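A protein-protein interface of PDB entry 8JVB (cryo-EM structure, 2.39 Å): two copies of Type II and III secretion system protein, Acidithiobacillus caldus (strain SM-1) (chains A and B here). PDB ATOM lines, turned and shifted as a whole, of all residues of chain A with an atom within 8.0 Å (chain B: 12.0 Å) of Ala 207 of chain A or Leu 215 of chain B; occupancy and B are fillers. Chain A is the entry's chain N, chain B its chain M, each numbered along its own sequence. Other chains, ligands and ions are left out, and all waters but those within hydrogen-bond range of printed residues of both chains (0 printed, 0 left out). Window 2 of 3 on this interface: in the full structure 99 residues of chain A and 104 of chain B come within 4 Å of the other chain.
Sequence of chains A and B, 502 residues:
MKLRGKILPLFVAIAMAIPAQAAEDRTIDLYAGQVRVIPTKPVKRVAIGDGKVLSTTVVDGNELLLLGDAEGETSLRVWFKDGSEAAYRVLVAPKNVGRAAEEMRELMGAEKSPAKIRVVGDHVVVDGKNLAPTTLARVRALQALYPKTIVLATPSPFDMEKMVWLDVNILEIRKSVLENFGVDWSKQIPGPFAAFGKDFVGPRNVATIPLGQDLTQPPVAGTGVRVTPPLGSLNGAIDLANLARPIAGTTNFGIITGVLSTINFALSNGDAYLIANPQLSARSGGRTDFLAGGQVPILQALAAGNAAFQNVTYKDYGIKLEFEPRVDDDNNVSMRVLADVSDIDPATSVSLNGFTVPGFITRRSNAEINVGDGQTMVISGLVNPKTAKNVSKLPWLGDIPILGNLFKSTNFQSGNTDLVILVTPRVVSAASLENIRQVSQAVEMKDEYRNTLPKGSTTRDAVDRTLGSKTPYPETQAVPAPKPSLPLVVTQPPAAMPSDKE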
ATOM      1  N   ARG A 204      20.197  -1.577   4.265  1.00  0.00           N
ATOM      2  CA  ARG A 204      19.848  -0.215   3.890  1.00  0.00           C
ATOM      3  C   ARG A 204      19.756  -0.097   2.377  1.00  0.00           C
ATOM      4  O   ARG A 204      20.533  -0.717   1.645  1.00  0.00           O
ATOM      5  CB  ARG A 204      20.879   0.780   4.424  1.00  0.00           C
ATOM      6  CG  ARG A 204      20.760   1.054   5.907  1.00  0.00           C
ATOM      7  CD  ARG A 204      20.091   2.388   6.162  1.00  0.00           C
ATOM      8  NE  ARG A 204      20.874   3.498   5.635  1.00  0.00           N
ATOM      9  CZ  ARG A 204      21.817   4.135   6.316  1.00  0.00           C
ATOM     10  NH1 ARG A 204      22.133   3.785   7.550  1.00  0.00           N
ATOM     11  NH2 ARG A 204      22.456   5.150   5.741  1.00  0.00           N
ATOM     12  N   ASN A 205      18.797   0.699   1.913  1.00  0.00           N
ATOM     13  CA  ASN A 205      18.636   1.003   0.497  1.00  0.00           C
ATOM     14  C   ASN A 205      19.084   2.439   0.265  1.00  0.00           C
ATOM     15  O   ASN A 205      18.530   3.369   0.861  1.00  0.00           O
ATOM     16  CB  ASN A 205      17.187   0.806   0.054  1.00  0.00           C
ATOM     17  CG  ASN A 205      16.719  -0.628   0.214  1.00  0.00           C
ATOM     18  OD1 ASN A 205      17.018  -1.485  -0.615  1.00  0.00           O
ATOM     19  ND2 ASN A 205      15.982  -0.894   1.286  1.00  0.00           N
ATOM     20  N   VAL A 206      20.087   2.617  -0.595  1.00  0.00           N
ATOM     21  CA  VAL A 206      20.687   3.921  -0.849  1.00  0.00           C
ATOM     22  C   VAL A 206      20.874   4.108  -2.347  1.00  0.00           C
ATOM     23  O   VAL A 206      20.856   3.153  -3.124  1.00  0.00           O
ATOM     24  CB  VAL A 206      22.040   4.089  -0.123  1.00  0.00           C
ATOM     25  CG1 VAL A 206      21.827   4.218   1.374  1.00  0.00           C
ATOM     26  CG2 VAL A 206      22.951   2.918  -0.432  1.00  0.00           C
ATOM     27  N   ALA A 207      21.048   5.365  -2.746  1.00  0.00           N
ATOM     28  CA  ALA A 207      21.351   5.703  -4.128  1.00  0.00           C
ATOM     29  C   ALA A 207      22.859   5.726  -4.338  1.00  0.00           C
ATOM     30  O   ALA A 207      23.606   6.222  -3.491  1.00  0.00           O
ATOM     31  CB  ALA A 207      20.749   7.058  -4.498  1.00  0.00           C
ATOM     32  N   THR A 208      23.301   5.187  -5.470  1.00  0.00           N
ATOM     33  CA  THR A 208      24.721   5.102  -5.772  1.00  0.00           C
ATOM     34  C   THR A 208      24.953   5.400  -7.247  1.00  0.00           C
ATOM     35  O   THR A 208      24.048   5.288  -8.077  1.00  0.00           O
ATOM     36  CB  THR A 208      25.295   3.723  -5.418  1.00  0.00           C
ATOM     37  OG1 THR A 208      26.726   3.764  -5.495  1.00  0.00           O
ATOM     38  CG2 THR A 208      24.773   2.662  -6.370  1.00  0.00           C
ATOM     39  N   ILE A 209      26.182   5.794  -7.558  1.00  0.00           N
ATOM     40  CA  ILE A 209      26.613   6.078  -8.920  1.00  0.00           C
ATOM     41  C   ILE A 209      27.770   5.141  -9.248  1.00  0.00           C
ATOM     42  O   ILE A 209      28.807   5.187  -8.580  1.00  0.00           O
ATOM     43  CB  ILE A 209      27.036   7.545  -9.101  1.00  0.00           C
ATOM     44  CG1 ILE A 209      25.896   8.485  -8.704  1.00  0.00           C
ATOM     45  CG2 ILE A 209      27.461   7.802 -10.536  1.00  0.00           C
ATOM     46  CD1 ILE A 209      26.082   9.135  -7.354  1.00  0.00           C
ATOM     47  N   PRO A 210      27.642   4.276 -10.250  1.00  0.00           N
ATOM     48  CA  PRO A 210      28.733   3.345 -10.565  1.00  0.00           C
ATOM     49  C   PRO A 210      29.977   4.076 -11.045  1.00  0.00           C
ATOM     50  O   PRO A 210      29.902   5.141 -11.660  1.00  0.00           O
ATOM     51  CB  PRO A 210      28.140   2.464 -11.671  1.00  0.00           C
ATOM     52  CG  PRO A 210      26.661   2.664 -11.584  1.00  0.00           C
ATOM     53  CD  PRO A 210      26.466   4.061 -11.105  1.00  0.00           C
ATOM     54  N   PRO A 218      21.181   9.764 -13.982  1.00  0.00           N
ATOM     55  CA  PRO A 218      20.544   9.598 -12.677  1.00  0.00           C
ATOM     56  C   PRO A 218      21.154   8.432 -11.929  1.00  0.00           C
ATOM     57  O   PRO A 218      21.657   7.470 -12.541  1.00  0.00           O
ATOM     58  CB  PRO A 218      19.072   9.336 -13.024  1.00  0.00           C
ATOM     59  CG  PRO A 218      18.960   9.301 -14.491  1.00  0.00           C
ATOM     60  CD  PRO A 218      20.240   9.698 -15.112  1.00  0.00           C
ATOM     61  N   PRO A 219      21.134   8.471 -10.600  1.00  0.00           N
ATOM     62  CA  PRO A 219      21.698   7.366  -9.819  1.00  0.00           C
ATOM     63  C   PRO A 219      20.837   6.117  -9.903  1.00  0.00           C
ATOM     64  O   PRO A 219      19.668   6.152 -10.294  1.00  0.00           O
ATOM     65  CB  PRO A 219      21.734   7.915  -8.385  1.00  0.00           C
ATOM     66  CG  PRO A 219      21.442   9.385  -8.504  1.00  0.00           C
ATOM     67  CD  PRO A 219      20.636   9.555  -9.741  1.00  0.00           C
ATOM     68  N   VAL A 220      21.440   4.994  -9.522  1.00  0.00           N
ATOM     69  CA  VAL A 220      20.756   3.706  -9.527  1.00  0.00           C
ATOM     70  C   VAL A 220      20.584   3.226  -8.093  1.00  0.00           C
ATOM     71  O   VAL A 220      21.038   3.880  -7.148  1.00  0.00           O
ATOM     72  CB  VAL A 220      21.519   2.670 -10.373  1.00  0.00           C
ATOM     73  CG1 VAL A 220      21.866   3.250 -11.729  1.00  0.00           C
ATOM     74  CG2 VAL A 220      22.774   2.218  -9.651  1.00  0.00           C
ATOM     75  N   ALA A 221      19.924   2.083  -7.920  1.00  0.00           N
ATOM     76  CA  ALA A 221      19.626   1.564  -6.592  1.00  0.00           C
ATOM     77  C   ALA A 221      20.836   0.826  -6.037  1.00  0.00           C
ATOM     78  O   ALA A 221      21.350  -0.103  -6.667  1.00  0.00           O
ATOM     79  CB  ALA A 221      18.411   0.641  -6.643  1.00  0.00           C
ATOM     80  N   GLY A 222      21.288   1.238  -4.853  1.00  0.00           N
ATOM     81  CA  GLY A 222      22.386   0.598  -4.168  1.00  0.00           C
ATOM     82  C   GLY A 222      21.959   0.069  -2.811  1.00  0.00           C
ATOM     83  O   GLY A 222      20.787   0.130  -2.429  1.00  0.00           O
ATOM     84  N   THR A 223      22.942  -0.451  -2.082  1.00  0.00           N
ATOM     85  CA  THR A 223      22.671  -1.066  -0.793  1.00  0.00           C
ATOM     86  C   THR A 223      23.867  -0.878   0.126  1.00  0.00           C
ATOM     87  O   THR A 223      24.975  -0.563  -0.314  1.00  0.00           O
ATOM     88  CB  THR A 223      22.353  -2.558  -0.935  1.00  0.00           C
ATOM     89  OG1 THR A 223      22.183  -3.138   0.363  1.00  0.00           O
ATOM     90  CG2 THR A 223      23.482  -3.275  -1.655  1.00  0.00           C
ATOM     91  N   THR B 208       8.725  -4.036  -5.245  1.00  0.00           N
ATOM     92  CA  THR B 208      10.161  -4.004  -5.011  1.00  0.00           C
ATOM     93  C   THR B 208      10.860  -3.350  -6.194  1.00  0.00           C
ATOM     94  O   THR B 208      10.326  -3.282  -7.302  1.00  0.00           O
ATOM     95  CB  THR B 208      10.727  -5.411  -4.775  1.00  0.00           C
ATOM     96  OG1 THR B 208      12.078  -5.313  -4.308  1.00  0.00           O
ATOM     97  CG2 THR B 208      10.701  -6.223  -6.058  1.00  0.00           C
ATOM     98  N   ILE B 209      12.067  -2.858  -5.937  1.00  0.00           N
ATOM     99  CA  ILE B 209      12.914  -2.238  -6.945  1.00  0.00           C
ATOM    100  C   ILE B 209      14.212  -3.034  -7.015  1.00  0.00           C
ATOM    101  O   ILE B 209      14.935  -3.123  -6.019  1.00  0.00           O
ATOM    102  CB  ILE B 209      13.202  -0.760  -6.636  1.00  0.00           C
ATOM    103  CG1 ILE B 209      11.893   0.021  -6.495  1.00  0.00           C
ATOM    104  CG2 ILE B 209      14.072  -0.150  -7.719  1.00  0.00           C
ATOM    105  CD1 ILE B 209      11.516   0.329  -5.066  1.00  0.00           C
ATOM    106  N   PRO B 210      14.546  -3.634  -8.156  1.00  0.00           N
ATOM    107  CA  PRO B 210      15.777  -4.429  -8.238  1.00  0.00           C
ATOM    108  C   PRO B 210      17.017  -3.569  -8.054  1.00  0.00           C
ATOM    109  O   PRO B 210      17.042  -2.388  -8.407  1.00  0.00           O
ATOM    110  CB  PRO B 210      15.720  -5.031  -9.648  1.00  0.00           C
ATOM    111  CG  PRO B 210      14.292  -4.899 -10.073  1.00  0.00           C
ATOM    112  CD  PRO B 210      13.780  -3.668  -9.411  1.00  0.00           C
ATOM    113  N   LEU B 211      18.055  -4.178  -7.489  1.00  0.00           N
ATOM    114  CA  LEU B 211      19.320  -3.484  -7.302  1.00  0.00           C
ATOM    115  C   LEU B 211      19.985  -3.221  -8.646  1.00  0.00           C
ATOM    116  O   LEU B 211      20.010  -4.086  -9.526  1.00  0.00           O
ATOM    117  CB  LEU B 211      20.249  -4.302  -6.407  1.00  0.00           C
ATOM    118  CG  LEU B 211      19.939  -4.304  -4.910  1.00  0.00           C
ATOM    119  CD1 LEU B 211      21.068  -4.958  -4.139  1.00  0.00           C
ATOM    120  CD2 LEU B 211      19.688  -2.894  -4.408  1.00  0.00           C
ATOM    121  N   GLY B 212      20.531  -2.018  -8.800  1.00  0.00           N
ATOM    122  CA  GLY B 212      21.142  -1.610 -10.044  1.00  0.00           C
ATOM    123  C   GLY B 212      20.197  -0.985 -11.043  1.00  0.00           C
ATOM    124  O   GLY B 212      20.651  -0.526 -12.099  1.00  0.00           O
ATOM    125  N   GLN B 213      18.902  -0.953 -10.750  1.00  0.00           N
ATOM    126  CA  GLN B 213      17.923  -0.339 -11.630  1.00  0.00           C
ATOM    127  C   GLN B 213      17.877   1.169 -11.409  1.00  0.00           C
ATOM    128  O   GLN B 213      18.256   1.683 -10.353  1.00  0.00           O
ATOM    129  CB  GLN B 213      16.540  -0.944 -11.391  1.00  0.00           C
ATOM    130  CG  GLN B 213      15.748  -1.222 -12.654  1.00  0.00           C
ATOM    131  CD  GLN B 213      14.269  -1.402 -12.380  1.00  0.00           C
ATOM    132  OE1 GLN B 213      13.656  -0.603 -11.673  1.00  0.00           O
ATOM    133  NE2 GLN B 213      13.686  -2.453 -12.943  1.00  0.00           N
ATOM    134  N   ASP B 214      17.404   1.879 -12.428  1.00  0.00           N
ATOM    135  CA  ASP B 214      17.225   3.317 -12.313  1.00  0.00           C
ATOM    136  C   ASP B 214      16.152   3.638 -11.277  1.00  0.00           C
ATOM    137  O   ASP B 214      15.171   2.908 -11.118  1.00  0.00           O
ATOM    138  CB  ASP B 214      16.846   3.918 -13.664  1.00  0.00           C
ATOM    139  CG  ASP B 214      17.197   5.387 -13.765  1.00  0.00           C
ATOM    140  OD1 ASP B 214      17.626   5.968 -12.748  1.00  0.00           O
ATOM    141  OD2 ASP B 214      17.039   5.961 -14.864  1.00  0.00           O
ATOM    142  N   LEU B 215      16.347   4.749 -10.569  1.00  0.00           N
ATOM    143  CA  LEU B 215      15.443   5.129  -9.493  1.00  0.00           C
ATOM    144  C   LEU B 215      14.128   5.712  -9.991  1.00  0.00           C
ATOM    145  O   LEU B 215      13.215   5.910  -9.182  1.00  0.00           O
ATOM    146  CB  LEU B 215      16.126   6.133  -8.563  1.00  0.00           C
ATOM    147  CG  LEU B 215      17.267   5.610  -7.687  1.00  0.00           C
ATOM    148  CD1 LEU B 215      17.342   6.394  -6.389  1.00  0.00           C
ATOM    149  CD2 LEU B 215      17.099   4.126  -7.400  1.00  0.00           C
ATOM    150  N   THR B 216      14.003   5.991 -11.287  1.00  0.00           N
ATOM    151  CA  THR B 216      12.777   6.554 -11.834  1.00  0.00           C
ATOM    152  C   THR B 216      11.831   5.509 -12.409  1.00  0.00           C
ATOM    153  O   THR B 216      10.654   5.818 -12.622  1.00  0.00           O
ATOM    154  CB  THR B 216      13.103   7.582 -12.925  1.00  0.00           C
ATOM    155  OG1 THR B 216      14.193   7.103 -13.724  1.00  0.00           O
ATOM    156  CG2 THR B 216      13.486   8.914 -12.302  1.00  0.00           C
ATOM    157  N   GLN B 217      12.309   4.295 -12.665  1.00  0.00           N
ATOM    158  CA  GLN B 217      11.462   3.270 -13.248  1.00  0.00           C
ATOM    159  C   GLN B 217      10.401   2.812 -12.248  1.00  0.00           C
ATOM    160  O   GLN B 217      10.630   2.825 -11.036  1.00  0.00           O
ATOM    161  CB  GLN B 217      12.297   2.077 -13.699  1.00  0.00           C
ATOM    162  CG  GLN B 217      13.598   2.455 -14.372  1.00  0.00           C
ATOM    163  CD  GLN B 217      13.917   1.561 -15.551  1.00  0.00           C
ATOM    164  OE1 GLN B 217      14.574   0.531 -15.403  1.00  0.00           O
ATOM    165  NE2 GLN B 217      13.454   1.950 -16.731  1.00  0.00           N
ATOM    166  N   PRO B 218       9.227   2.412 -12.733  1.00  0.00           N
ATOM    167  CA  PRO B 218       8.196   1.916 -11.825  1.00  0.00           C
ATOM    168  C   PRO B 218       8.632   0.621 -11.174  1.00  0.00           C
ATOM    169  O   PRO B 218       9.426  -0.148 -11.750  1.00  0.00           O
ATOM    170  CB  PRO B 218       6.980   1.706 -12.738  1.00  0.00           C
ATOM    171  CG  PRO B 218       7.398   2.025 -14.114  1.00  0.00           C
ATOM    172  CD  PRO B 218       8.759   2.597 -14.116  1.00  0.00           C
ATOM    173  N   PRO B 219       8.142   0.335  -9.972  1.00  0.00           N
ATOM    174  CA  PRO B 219       8.518  -0.910  -9.296  1.00  0.00           C
ATOM    175  C   PRO B 219       7.891  -2.125  -9.961  1.00  0.00           C
ATOM    176  O   PRO B 219       6.939  -2.029 -10.739  1.00  0.00           O
ATOM    177  CB  PRO B 219       7.982  -0.725  -7.869  1.00  0.00           C
ATOM    178  CG  PRO B 219       7.584   0.721  -7.767  1.00  0.00           C
ATOM    179  CD  PRO B 219       7.251   1.163  -9.147  1.00  0.00           C
ATOM    180  N   VAL B 220       8.446  -3.290  -9.636  1.00  0.00           N
ATOM    181  CA  VAL B 220       7.962  -4.556 -10.172  1.00  0.00           C
ATOM    182  C   VAL B 220       7.351  -5.377  -9.043  1.00  0.00           C
ATOM    183  O   VAL B 220       7.365  -4.959  -7.881  1.00  0.00           O
ATOM    184  CB  VAL B 220       9.088  -5.334 -10.877  1.00  0.00           C
ATOM    185  CG1 VAL B 220       9.821  -4.432 -11.850  1.00  0.00           C
ATOM    186  CG2 VAL B 220      10.051  -5.912  -9.858  1.00  0.00           C
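The backbone carbonyl oxygen (O) of Ala 221 of chain A is in hydrogen-bond range of the backbone NH (N) of Gly 212 of chain B.
The backbone NH (N) of Ala 221 of chain A lies within hydrogen-bond range of the backbone carbonyl oxygen (O) of Gln 213 of chain B (3.0 Å).
O of Pro 219 of chain A lies close to OD1 of Asp 214 of chain B (3.2 Å).
Ala 207 of chain A touches just one residue of chain B: Leu 215 (3.95 Å).
Printed residues of chain A within 4 Å of Leu 215 of chain B: Ala 207, Pro 219, Val 220 and Ala 221.
No residue of chain B comes within 4 Å of Thr 208 of chain A.
Of chain B, only Asp 214 (3.7 Å) comes within 4 Å of Pro 218 of chain A.
Of chain B, only Asp 214 and Leu 215 come within 4 Å of Pro 219 of chain A.
Of chain B, only Gly 212, Gln 213 and Leu 215 come within 4 Å of Val 220 of chain A.
Of chain B, only Pro 210 (3.8 Å), Leu 211 (3.9 Å), Gly 212 (3.0 Å), Gln 213 (3.0 Å) and Leu 215 (3.5 Å) come within 4 Å of Ala 221 of chain A.
Gly 222 of chain A touches just one residue of chain B: Leu 211 (3.8 Å).
Printed residues of chain A within 4 Å of Pro 210 of chain B: Ala 221 (3.8 Å).
Printed residues of chain A within 4 Å of Asp 214 of chain B: Pro 218 and Pro 219.
Of the printed residues of chain A, Gln 213 of chain B touches Val 220 (3.3 Å) and Ala 221 (3.0 Å).
Pro 210 of chain A touches none of the printed residues of chain B.
The nearest residue of chain B that does not touch Ala 207 of chain A is Gln 213 of chain B (8.0 Å).
Positions printed for both chains: 208, 209, 210, 218, 219 and 220.
Of the 14 pairs that touch across the chains among the printed residues, none has its exchanged pair printed and touching as well.
OG1 of Thr 216 of chain B lies within hydrogen-bond range of OD2 of Asp 214 of chain B, at 3.3 Å.
The backbone carbonyl oxygen of Arg 204 of chain A is in hydrogen-bond range of the side-chain hydroxyl of Thr 223 of chain A (3.2 Å).
O of Val 206 of chain A lies within hydrogen-bond range of N of Gly 222 of chain A (2.6 Å).
The backbone NH (N) of Val 220 of chain A is in hydrogen-bond range of the backbone carbonyl oxygen (O) of Thr 208 of chain A (3.0 Å).
Hydrophobic or aromatic side chains of chain A within 4 Å of the printed part of chain B: Ala 207, Pro 218, Val 220 and Ala 221.
Hydrophobic or aromatic side chains of chain B that line the printed part of chain A: Leu 211 and Leu 215.
Along chain B the printed residues that touch a printed residue of chain A span positions 210 to 215.
Among the printed residues, no Asp or Glu carboxylate lies within 4 Å of a Lys or Arg side-chain nitrogen of the other chain.
Among the printed residues, pairs that only touch across the chains: Val 220 of chain A with Gln 213 of chain B, Ala 221 of chain A with Leu 215 of chain B, Pro 219 of chain A with Leu 215 of chain B, Val 220 of chain A with Leu 215 of chain B, Pro 218 of chain A with Asp 214 of chain B, Val 220 of chain A with Gly 212 of chain B, Ala 221 of chain A with Pro 210 of chain B, Gly 222 of chain A with Leu 211 of chain B, Thr 223 of chain A with Leu 211 of chain B, Ala 221 of chain A with Leu 211 of chain B and Ala 207 of chain A with Leu 215 of chain B.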
